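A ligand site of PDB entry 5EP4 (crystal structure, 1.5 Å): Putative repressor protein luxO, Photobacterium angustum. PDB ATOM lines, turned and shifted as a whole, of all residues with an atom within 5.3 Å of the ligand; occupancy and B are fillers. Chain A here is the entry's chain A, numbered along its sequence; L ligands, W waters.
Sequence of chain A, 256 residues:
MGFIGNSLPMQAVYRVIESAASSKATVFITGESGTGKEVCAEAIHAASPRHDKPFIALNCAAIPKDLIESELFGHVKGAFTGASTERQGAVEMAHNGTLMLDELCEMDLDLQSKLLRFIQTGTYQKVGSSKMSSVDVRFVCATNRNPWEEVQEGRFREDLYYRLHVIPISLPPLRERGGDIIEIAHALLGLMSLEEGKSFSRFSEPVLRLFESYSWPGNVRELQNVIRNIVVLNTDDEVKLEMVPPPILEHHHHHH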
ATOM      1  N   GLY A   2       8.918  25.945  -7.919  1.00  0.00           N
ATOM      2  CA  GLY A   2       9.221  27.370  -7.955  1.00  0.00           C
ATOM      3  C   GLY A   2      10.597  27.755  -8.484  1.00  0.00           C
ATOM      4  O   GLY A   2      10.959  28.906  -8.452  1.00  0.00           O
ATOM      5  N   PHE A   3      11.366  26.785  -8.950  1.00  0.00           N
ATOM      6  CA  PHE A   3      12.632  27.108  -9.600  1.00  0.00           C
ATOM      7  C   PHE A   3      12.384  27.864 -10.884  1.00  0.00           C
ATOM      8  O   PHE A   3      11.597  27.441 -11.737  1.00  0.00           O
ATOM      9  CB  PHE A   3      13.389  25.844  -9.917  1.00  0.00           C
ATOM     10  CG  PHE A   3      14.380  25.455  -8.877  1.00  0.00           C
ATOM     11  CD1 PHE A   3      15.067  26.431  -8.172  1.00  0.00           C
ATOM     12  CD2 PHE A   3      14.600  24.130  -8.580  1.00  0.00           C
ATOM     13  CE1 PHE A   3      15.976  26.087  -7.196  1.00  0.00           C
ATOM     14  CE2 PHE A   3      15.541  23.811  -7.690  1.00  0.00           C
ATOM     15  CZ  PHE A   3      16.248  24.781  -7.006  1.00  0.00           C
ATOM     16  N   ILE A   4      13.076  28.965 -11.054  1.00  0.00           N
ATOM     17  CA  ILE A   4      13.116  29.647 -12.331  1.00  0.00           C
ATOM     18  C   ILE A   4      14.571  29.588 -12.770  1.00  0.00           C
ATOM     19  O   ILE A   4      15.491  29.666 -11.938  1.00  0.00           O
ATOM     20  CB  ILE A   4      12.578  31.096 -12.218  1.00  0.00           C
ATOM     21  CG1 ILE A   4      11.070  31.001 -11.936  1.00  0.00           C
ATOM     22  CG2 ILE A   4      12.815  31.952 -13.471  1.00  0.00           C
ATOM     23  CD1 ILE A   4      10.448  32.267 -11.481  1.00  0.00           C
ATOM     24  N   MET A  10      22.102  25.411 -13.128  1.00  0.00           N
ATOM     25  CA  MET A  10      20.811  25.027 -12.575  1.00  0.00           C
ATOM     26  C   MET A  10      20.260  23.810 -13.277  1.00  0.00           C
ATOM     27  O   MET A  10      19.580  22.981 -12.621  1.00  0.00           O
ATOM     28  CB  MET A  10      19.807  26.180 -12.669  1.00  0.00           C
ATOM     29  CG  MET A  10      20.100  27.360 -11.740  1.00  0.00           C
ATOM     30  SD  MET A  10      20.135  26.870  -9.974  1.00  0.00           S
ATOM     31  CE  MET A  10      18.456  26.439  -9.714  1.00  0.00           C
ATOM     32  N   GLU A  32      25.180  29.600  -0.761  1.00  0.00           N
ATOM     33  CA  GLU A  32      25.195  30.848  -0.022  1.00  0.00           C
ATOM     34  C   GLU A  32      23.795  31.253   0.430  1.00  0.00           C
ATOM     35  O   GLU A  32      22.780  30.772  -0.053  1.00  0.00           O
ATOM     36  CB  GLU A  32      25.828  31.946  -0.906  1.00  0.00           C
ATOM     37  CG  GLU A  32      27.294  31.700  -1.256  1.00  0.00           C
ATOM     38  CD  GLU A  32      27.838  32.716  -2.278  1.00  0.00           C
ATOM     39  OE1 GLU A  32      27.095  33.653  -2.647  1.00  0.00           O
ATOM     40  OE2 GLU A  32      28.970  32.520  -2.733  1.00  0.00           O
ATOM     41  N   SER A  33      23.748  32.198   1.384  1.00  0.00           N
ATOM     42  CA  SER A  33      22.456  32.682   1.822  1.00  0.00           C
ATOM     43  C   SER A  33      21.662  33.218   0.626  1.00  0.00           C
ATOM     44  O   SER A  33      22.216  33.798  -0.320  1.00  0.00           O
ATOM     45  CB  SER A  33      22.590  33.759   2.906  1.00  0.00           C
ATOM     46  OG  SER A  33      23.069  34.980   2.376  1.00  0.00           O
ATOM     47  N   GLY A  34      20.388  32.908   0.658  1.00  0.00           N
ATOM     48  CA  GLY A  34      19.427  33.316  -0.345  1.00  0.00           C
ATOM     49  C   GLY A  34      19.517  32.618  -1.676  1.00  0.00           C
ATOM     50  O   GLY A  34      18.998  33.143  -2.640  1.00  0.00           O
ATOM     51  N   THR A  35      20.096  31.409  -1.758  1.00  0.00           N
ATOM     52  CA  THR A  35      20.245  30.743  -3.061  1.00  0.00           C
ATOM     53  C   THR A  35      19.082  29.834  -3.431  1.00  0.00           C
ATOM     54  O   THR A  35      19.072  29.282  -4.528  1.00  0.00           O
ATOM     55  CB  THR A  35      21.580  29.944  -3.136  1.00  0.00           C
ATOM     56  OG1 THR A  35      21.759  29.167  -1.937  1.00  0.00           O
ATOM     57  CG2 THR A  35      22.756  30.883  -3.283  1.00  0.00           C
ATOM     58  N   GLY A  36      18.090  29.672  -2.568  1.00  0.00           N
ATOM     59  CA  GLY A  36      16.918  28.889  -2.867  1.00  0.00           C
ATOM     60  C   GLY A  36      16.923  27.469  -2.337  1.00  0.00           C
ATOM     61  O   GLY A  36      16.438  26.593  -3.020  1.00  0.00           O
ATOM     62  N   LYS A  37      17.516  27.241  -1.165  1.00  0.00           N
ATOM     63  CA  LYS A  37      17.582  25.873  -0.639  1.00  0.00           C
ATOM     64  C   LYS A  37      16.208  25.302  -0.276  1.00  0.00           C
ATOM     65  O   LYS A  37      15.971  24.112  -0.508  1.00  0.00           O
ATOM     66  CB  LYS A  37      18.530  25.834   0.548  1.00  0.00           C
ATOM     67  CG  LYS A  37      19.948  26.321   0.106  1.00  0.00           C
ATOM     68  CD  LYS A  37      20.946  26.184   1.262  1.00  0.00           C
ATOM     69  CE  LYS A  37      20.805  27.323   2.228  1.00  0.00           C
ATOM     70  NZ  LYS A  37      21.237  28.594   1.530  1.00  0.00           N
ATOM     71  N   GLU A  38      15.253  26.129   0.196  1.00  0.00           N
ATOM     72  CA  GLU A  38      13.928  25.592   0.521  1.00  0.00           C
ATOM     73  C   GLU A  38      13.099  25.362  -0.752  1.00  0.00           C
ATOM     74  O   GLU A  38      12.417  24.353  -0.903  1.00  0.00           O
ATOM     75  CB  GLU A  38      13.220  26.500   1.519  1.00  0.00           C
ATOM     76  CG  GLU A  38      11.830  25.975   1.840  1.00  0.00           C
ATOM     77  CD  GLU A  38      11.189  26.666   3.015  1.00  0.00           C
ATOM     78  OE1 GLU A  38       9.945  26.608   3.115  1.00  0.00           O
ATOM     79  OE2 GLU A  38      11.908  27.291   3.804  1.00  0.00           O
ATOM     80  N   VAL A  39      13.251  26.257  -1.756  1.00  0.00           N
ATOM     81  CA  VAL A  39      12.656  25.991  -3.063  1.00  0.00           C
ATOM     82  C   VAL A  39      13.189  24.694  -3.637  1.00  0.00           C
ATOM     83  O   VAL A  39      12.472  23.927  -4.240  1.00  0.00           O
ATOM     84  CB  VAL A  39      12.977  27.176  -4.005  1.00  0.00           C
ATOM     85  CG1 VAL A  39      12.814  26.788  -5.511  1.00  0.00           C
ATOM     86  CG2 VAL A  39      12.134  28.351  -3.660  1.00  0.00           C
ATOM     87  N   CYS A  40      14.507  24.452  -3.491  1.00  0.00           N
ATOM     88  CA  CYS A  40      15.065  23.236  -4.022  1.00  0.00           C
ATOM     89  C   CYS A  40      14.459  22.026  -3.307  1.00  0.00           C
ATOM     90  O   CYS A  40      14.137  21.003  -3.925  1.00  0.00           O
ATOM     91  CB  CYS A  40      16.595  23.312  -3.847  1.00  0.00           C
ATOM     92  SG  CYS A  40      17.438  21.937  -4.638  1.00  0.00           S
ATOM     93  N   MET A 100      12.073  18.830   5.676  1.00  0.00           N
ATOM     94  CA  MET A 100      13.278  19.634   5.450  1.00  0.00           C
ATOM     95  C   MET A 100      13.860  20.124   6.762  1.00  0.00           C
ATOM     96  O   MET A 100      13.170  20.818   7.524  1.00  0.00           O
ATOM     97  CB  MET A 100      13.031  20.841   4.517  1.00  0.00           C
ATOM     98  CG  MET A 100      14.334  21.598   4.182  1.00  0.00           C
ATOM     99  SD  MET A 100      13.879  23.201   3.485  1.00  0.00           S
ATOM    100  CE  MET A 100      15.570  23.721   3.035  1.00  0.00           C
ATOM    101  N   ASP A 102      15.984  22.606   7.741  1.00  0.00           N
ATOM    102  CA  ASP A 102      16.613  23.813   7.180  1.00  0.00           C
ATOM    103  C   ASP A 102      17.492  24.513   8.201  1.00  0.00           C
ATOM    104  O   ASP A 102      17.083  24.761   9.344  1.00  0.00           O
ATOM    105  CB  ASP A 102      15.497  24.752   6.720  1.00  0.00           C
ATOM    106  CG  ASP A 102      16.012  26.022   6.059  1.00  0.00           C
ATOM    107  OD1 ASP A 102      16.881  25.912   5.187  1.00  0.00           O
ATOM    108  OD2 ASP A 102      15.517  27.105   6.420  1.00  0.00           O
ATOM    109  N   GLU A 103      18.676  24.909   7.763  1.00  0.00           N
ATOM    110  CA  GLU A 103      19.679  25.511   8.629  1.00  0.00           C
ATOM    111  C   GLU A 103      19.937  24.663   9.878  1.00  0.00           C
ATOM    112  O   GLU A 103      20.005  25.127  11.020  1.00  0.00           O
ATOM    113  CB  GLU A 103      19.292  26.976   8.973  1.00  0.00           C
ATOM    114  CG  GLU A 103      19.104  27.885   7.701  1.00  0.00           C
ATOM    115  CD  GLU A 103      20.350  27.881   6.741  1.00  0.00           C
ATOM    116  OE1 GLU A 103      21.461  27.568   7.191  1.00  0.00           O
ATOM    117  OE2 GLU A 103      20.192  28.153   5.517  1.00  0.00           O
ATOM    118  N   ASN A 144      23.523  27.111   5.143  1.00  0.00           N
ATOM    119  CA  ASN A 144      24.358  28.218   4.655  1.00  0.00           C
ATOM    120  C   ASN A 144      25.806  28.101   5.069  1.00  0.00           C
ATOM    121  O   ASN A 144      26.661  28.859   4.576  1.00  0.00           O
ATOM    122  CB  ASN A 144      23.943  29.560   5.244  1.00  0.00           C
ATOM    123  CG  ASN A 144      22.639  30.000   4.788  1.00  0.00           C
ATOM    124  OD1 ASN A 144      22.142  29.556   3.758  1.00  0.00           O
ATOM    125  ND2 ASN A 144      22.057  30.908   5.516  1.00  0.00           N
ATOM    126  N   ARG A 177      24.713  32.401 -12.599  1.00  0.00           N
ATOM    127  CA  ARG A 177      23.542  31.783 -13.225  1.00  0.00           C
ATOM    128  C   ARG A 177      23.108  32.403 -14.552  1.00  0.00           C
ATOM    129  O   ARG A 177      22.026  32.102 -15.044  1.00  0.00           O
ATOM    130  CB  ARG A 177      22.352  31.779 -12.245  1.00  0.00           C
ATOM    131  CG  ARG A 177      22.569  30.917 -11.040  1.00  0.00           C
ATOM    132  CD  ARG A 177      21.274  30.820 -10.305  1.00  0.00           C
ATOM    133  NE  ARG A 177      21.505  30.467  -8.917  1.00  0.00           N
ATOM    134  CZ  ARG A 177      20.508  30.211  -8.069  1.00  0.00           C
ATOM    135  NH1 ARG A 177      19.236  30.311  -8.432  1.00  0.00           N
ATOM    136  NH2 ARG A 177      20.838  29.949  -6.825  1.00  0.00           N
ATOM    137  N   ILE A 184      14.556  35.489 -13.335  1.00  0.00           N
ATOM    138  CA  ILE A 184      13.989  35.628 -11.986  1.00  0.00           C
ATOM    139  C   ILE A 184      13.530  37.059 -11.746  1.00  0.00           C
ATOM    140  O   ILE A 184      12.422  37.292 -11.222  1.00  0.00           O
ATOM    141  CB  ILE A 184      15.006  35.182 -10.943  1.00  0.00           C
ATOM    142  CG1 ILE A 184      15.348  33.706 -11.104  1.00  0.00           C
ATOM    143  CG2 ILE A 184      14.498  35.457  -9.564  1.00  0.00           C
ATOM    144  CD1 ILE A 184      16.578  33.371 -10.333  1.00  0.00           C
ATOM    145  N   VAL A 220      19.241  35.350  -4.335  1.00  0.00           N
ATOM    146  CA  VAL A 220      17.892  35.619  -4.769  1.00  0.00           C
ATOM    147  C   VAL A 220      17.155  36.444  -3.727  1.00  0.00           C
ATOM    148  O   VAL A 220      16.297  37.260  -4.100  1.00  0.00           O
ATOM    149  CB  VAL A 220      17.128  34.318  -5.112  1.00  0.00           C
ATOM    150  CG1 VAL A 220      15.768  34.605  -5.654  1.00  0.00           C
ATOM    151  CG2 VAL A 220      17.939  33.526  -6.146  1.00  0.00           C
ATOM    152  N   ARG A 221      17.442  36.282  -2.420  1.00  0.00           N
ATOM    153  CA  ARG A 221      16.738  37.163  -1.486  1.00  0.00           C
ATOM    154  C   ARG A 221      17.098  38.627  -1.732  1.00  0.00           C
ATOM    155  O   ARG A 221      16.201  39.469  -1.688  1.00  0.00           O
ATOM    156  CB  ARG A 221      17.093  36.854  -0.037  1.00  0.00           C
ATOM    157  CG  ARG A 221      16.377  37.811   0.950  1.00  0.00           C
ATOM    158  CD  ARG A 221      16.443  37.246   2.403  1.00  0.00           C
ATOM    159  NE  ARG A 221      15.897  35.885   2.493  1.00  0.00           N
ATOM    160  CZ  ARG A 221      14.588  35.641   2.500  1.00  0.00           C
ATOM    161  NH1 ARG A 221      13.701  36.660   2.469  1.00  0.00           N
ATOM    162  NH2 ARG A 221      14.154  34.396   2.526  1.00  0.00           N
ATOM    163  N   GLN A 224      15.119  39.756  -4.628  1.00  0.00           N
ATOM    164  CA  GLN A 224      13.738  39.997  -4.204  1.00  0.00           C
ATOM    165  C   GLN A 224      13.632  41.329  -3.474  1.00  0.00           C
ATOM    166  O   GLN A 224      12.729  42.118  -3.741  1.00  0.00           O
ATOM    167  CB  GLN A 224      13.241  38.877  -3.281  1.00  0.00           C
ATOM    168  CG  GLN A 224      12.939  37.622  -4.001  1.00  0.00           C
ATOM    169  CD  GLN A 224      12.488  36.569  -3.007  1.00  0.00           C
ATOM    170  OE1 GLN A 224      12.930  36.571  -1.850  1.00  0.00           O
ATOM    171  NE2 GLN A 224      11.567  35.698  -3.415  1.00  0.00           N
HETATM  172  P1  LIG L   1      17.303  32.381   2.866  1.00  0.00           P
HETATM  173  O1  LIG L   1      15.808  32.210   3.118  1.00  0.00           O
HETATM  174  O2  LIG L   1      17.692  33.827   2.443  1.00  0.00           O
HETATM  175  O3  LIG L   1      18.153  31.773   3.972  1.00  0.00           O
HETATM  176  P2  LIG L   1      17.290  29.801   1.145  1.00  0.00           P
HETATM  177  O4  LIG L   1      16.649  28.681   1.958  1.00  0.00           O
HETATM  178  O5  LIG L   1      18.515  29.430   0.340  1.00  0.00           O
HETATM  179  O6  LIG L   1      17.765  31.224   1.799  1.00  0.00           O
HETATM  180  P3  LIG L   1      14.593  30.018  -0.060  1.00  0.00           P
HETATM  181  O7  LIG L   1      13.903  30.349   1.247  1.00  0.00           O
HETATM  182  O8  LIG L   1      14.399  28.794  -0.827  1.00  0.00           O
HETATM  183  O9  LIG L   1      16.164  30.364   0.124  1.00  0.00           O
HETATM  184  O10 LIG L   1      14.206  31.157  -1.154  1.00  0.00           O
HETATM  185  C1  LIG L   1      14.294  32.565  -0.852  1.00  0.00           C
HETATM  186  C2  LIG L   1      13.204  33.271  -1.655  1.00  0.00           C
HETATM  187  O11 LIG L   1      13.702  33.324  -3.004  1.00  0.00           O
HETATM  188  C3  LIG L   1      11.872  32.552  -1.766  1.00  0.00           C
HETATM  189  O12 LIG L   1      10.795  33.551  -1.757  1.00  0.00           O
HETATM  190  C4  LIG L   1      11.890  31.836  -3.124  1.00  0.00           C
HETATM  191  O13 LIG L   1      10.629  31.702  -3.809  1.00  0.00           O
HETATM  192  C5  LIG L   1      12.769  32.762  -3.933  1.00  0.00           C
HETATM  193  N1  LIG L   1      13.600  31.978  -4.898  1.00  0.00           N
HETATM  194  C6  LIG L   1      14.749  31.340  -4.613  1.00  0.00           C
HETATM  195  N2  LIG L   1      15.268  30.686  -5.661  1.00  0.00           N
HETATM  196  C7  LIG L   1      14.437  30.985  -6.689  1.00  0.00           C
HETATM  197  C8  LIG L   1      14.405  30.660  -8.146  1.00  0.00           C
HETATM  198  N3  LIG L   1      15.363  29.889  -8.721  1.00  0.00           N
HETATM  199  N4  LIG L   1      13.374  31.140  -8.848  1.00  0.00           N
HETATM  200  C9  LIG L   1      12.422  31.923  -8.327  1.00  0.00           C
HETATM  201  N5  LIG L   1      12.391  32.257  -7.029  1.00  0.00           N
HETATM  202  C10 LIG L   1      13.375  31.825  -6.197  1.00  0.00           C
HETATM  203  O   HOH W   1      17.218  29.237  -6.613  1.00  0.00           O
HETATM  204  O   HOH W   2       8.304  32.510  -1.243  1.00  0.00           O
HETATM  205  O   HOH W   3      17.457  30.704   6.176  1.00  0.00           O
HETATM  206  O   HOH W   4       9.376  29.799  -6.085  1.00  0.00           O
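N4 of the ligand lies close to O of Gly 2 (3.3 Å).
Phe 3 touches the ligand.
Arg 177 touches the ligand (NH1 to N3, 3.9 Å).
Ile 184 touches the ligand (CG1 to N4, 3.9 Å).
CG1 of Val 220 touches N1 of the ligand, 3.5 Å away.
Hydrophobic or aromatic side chains within 4 Å of the ligand: Phe 3, Ile 4, Val 39, Ile 184 and Val 220.
14 residues have an atom within 4 Å of the ligand: Gly 2, Phe 3, Ile 4, Gly 34, Thr 35, Gly 36, Lys 37, Glu 38, Val 39, Arg 177, Ile 184, Val 220, Arg 221 and Gln 224.
Along chain A the residues within 4 Å of the ligand span positions 2 to 224.
The nearest printed residue that does not touch the ligand is Asp 102 (4.3 Å).
Water W1 lies within hydrogen-bond range of a nitrogen (N2) of the ligand, the backbone carbonyl oxygen of Thr 35 and the guanidinium group of Arg 177.
Water W4 bridges the backbone carbonyl oxygen (O) of Gly 2 (3.0 Å) and an oxygen (O13) of the ligand (3.2 Å).
N of Gly 36 lies within hydrogen-bond range of O5 of the ligand.
N of Glu 38 lies within hydrogen-bond range of O8 of the ligand (3.0 Å).
An oxygen (O5) of the ligand lies within salt-bridge range of the side-chain amino group (NZ) of Lys 37.
N of Gly 34 sits at hydrogen-bond distance from O6 of the ligand (3.3 Å).
The backbone carbonyl oxygen (O) of Ile 4 sits at hydrogen-bond distance from a nitrogen (N3) of the ligand.
The side-chain amide nitrogen of Gln 224 lies within hydrogen-bond range of an oxygen (O12) of the ligand, 2.8 Å away.
The backbone NH (N) of Thr 35 sits at hydrogen-bond distance from an oxygen (O5) of the ligand (3.3 Å).
N of Lys 37 sits at hydrogen-bond distance from O5 of the ligand (2.8 Å).
An oxygen (O8) of the ligand is in hydrogen-bond range of the backbone NH of Val 39 (2.9 Å).
An oxygen (O2) of the ligand is in salt-bridge range of the guanidinium group (NE) of Arg 221.
A nitrogen (N4) of the ligand lies within hydrogen-bond range of the backbone NH (N) of Ile 4 (3.1 Å).
The backbone carbonyl oxygen (O) of Thr 35 is in hydrogen-bond range of the guanidinium group (NH2) of Arg 177 (3.0 Å).
O of Gly 34 lies within hydrogen-bond range of N of Val 220, 2.8 Å away.
O of Glu 32 lies within hydrogen-bond range of NZ of Lys 37 (3.1 Å).
The side-chain amide oxygen (OD1) of Asn 144 lies within hydrogen-bond range of the side-chain amino group (NZ) of Lys 37 (2.6 Å).
The side-chain hydroxyl of Thr 35 lies within hydrogen-bond range of the backbone carbonyl oxygen of Glu 32.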
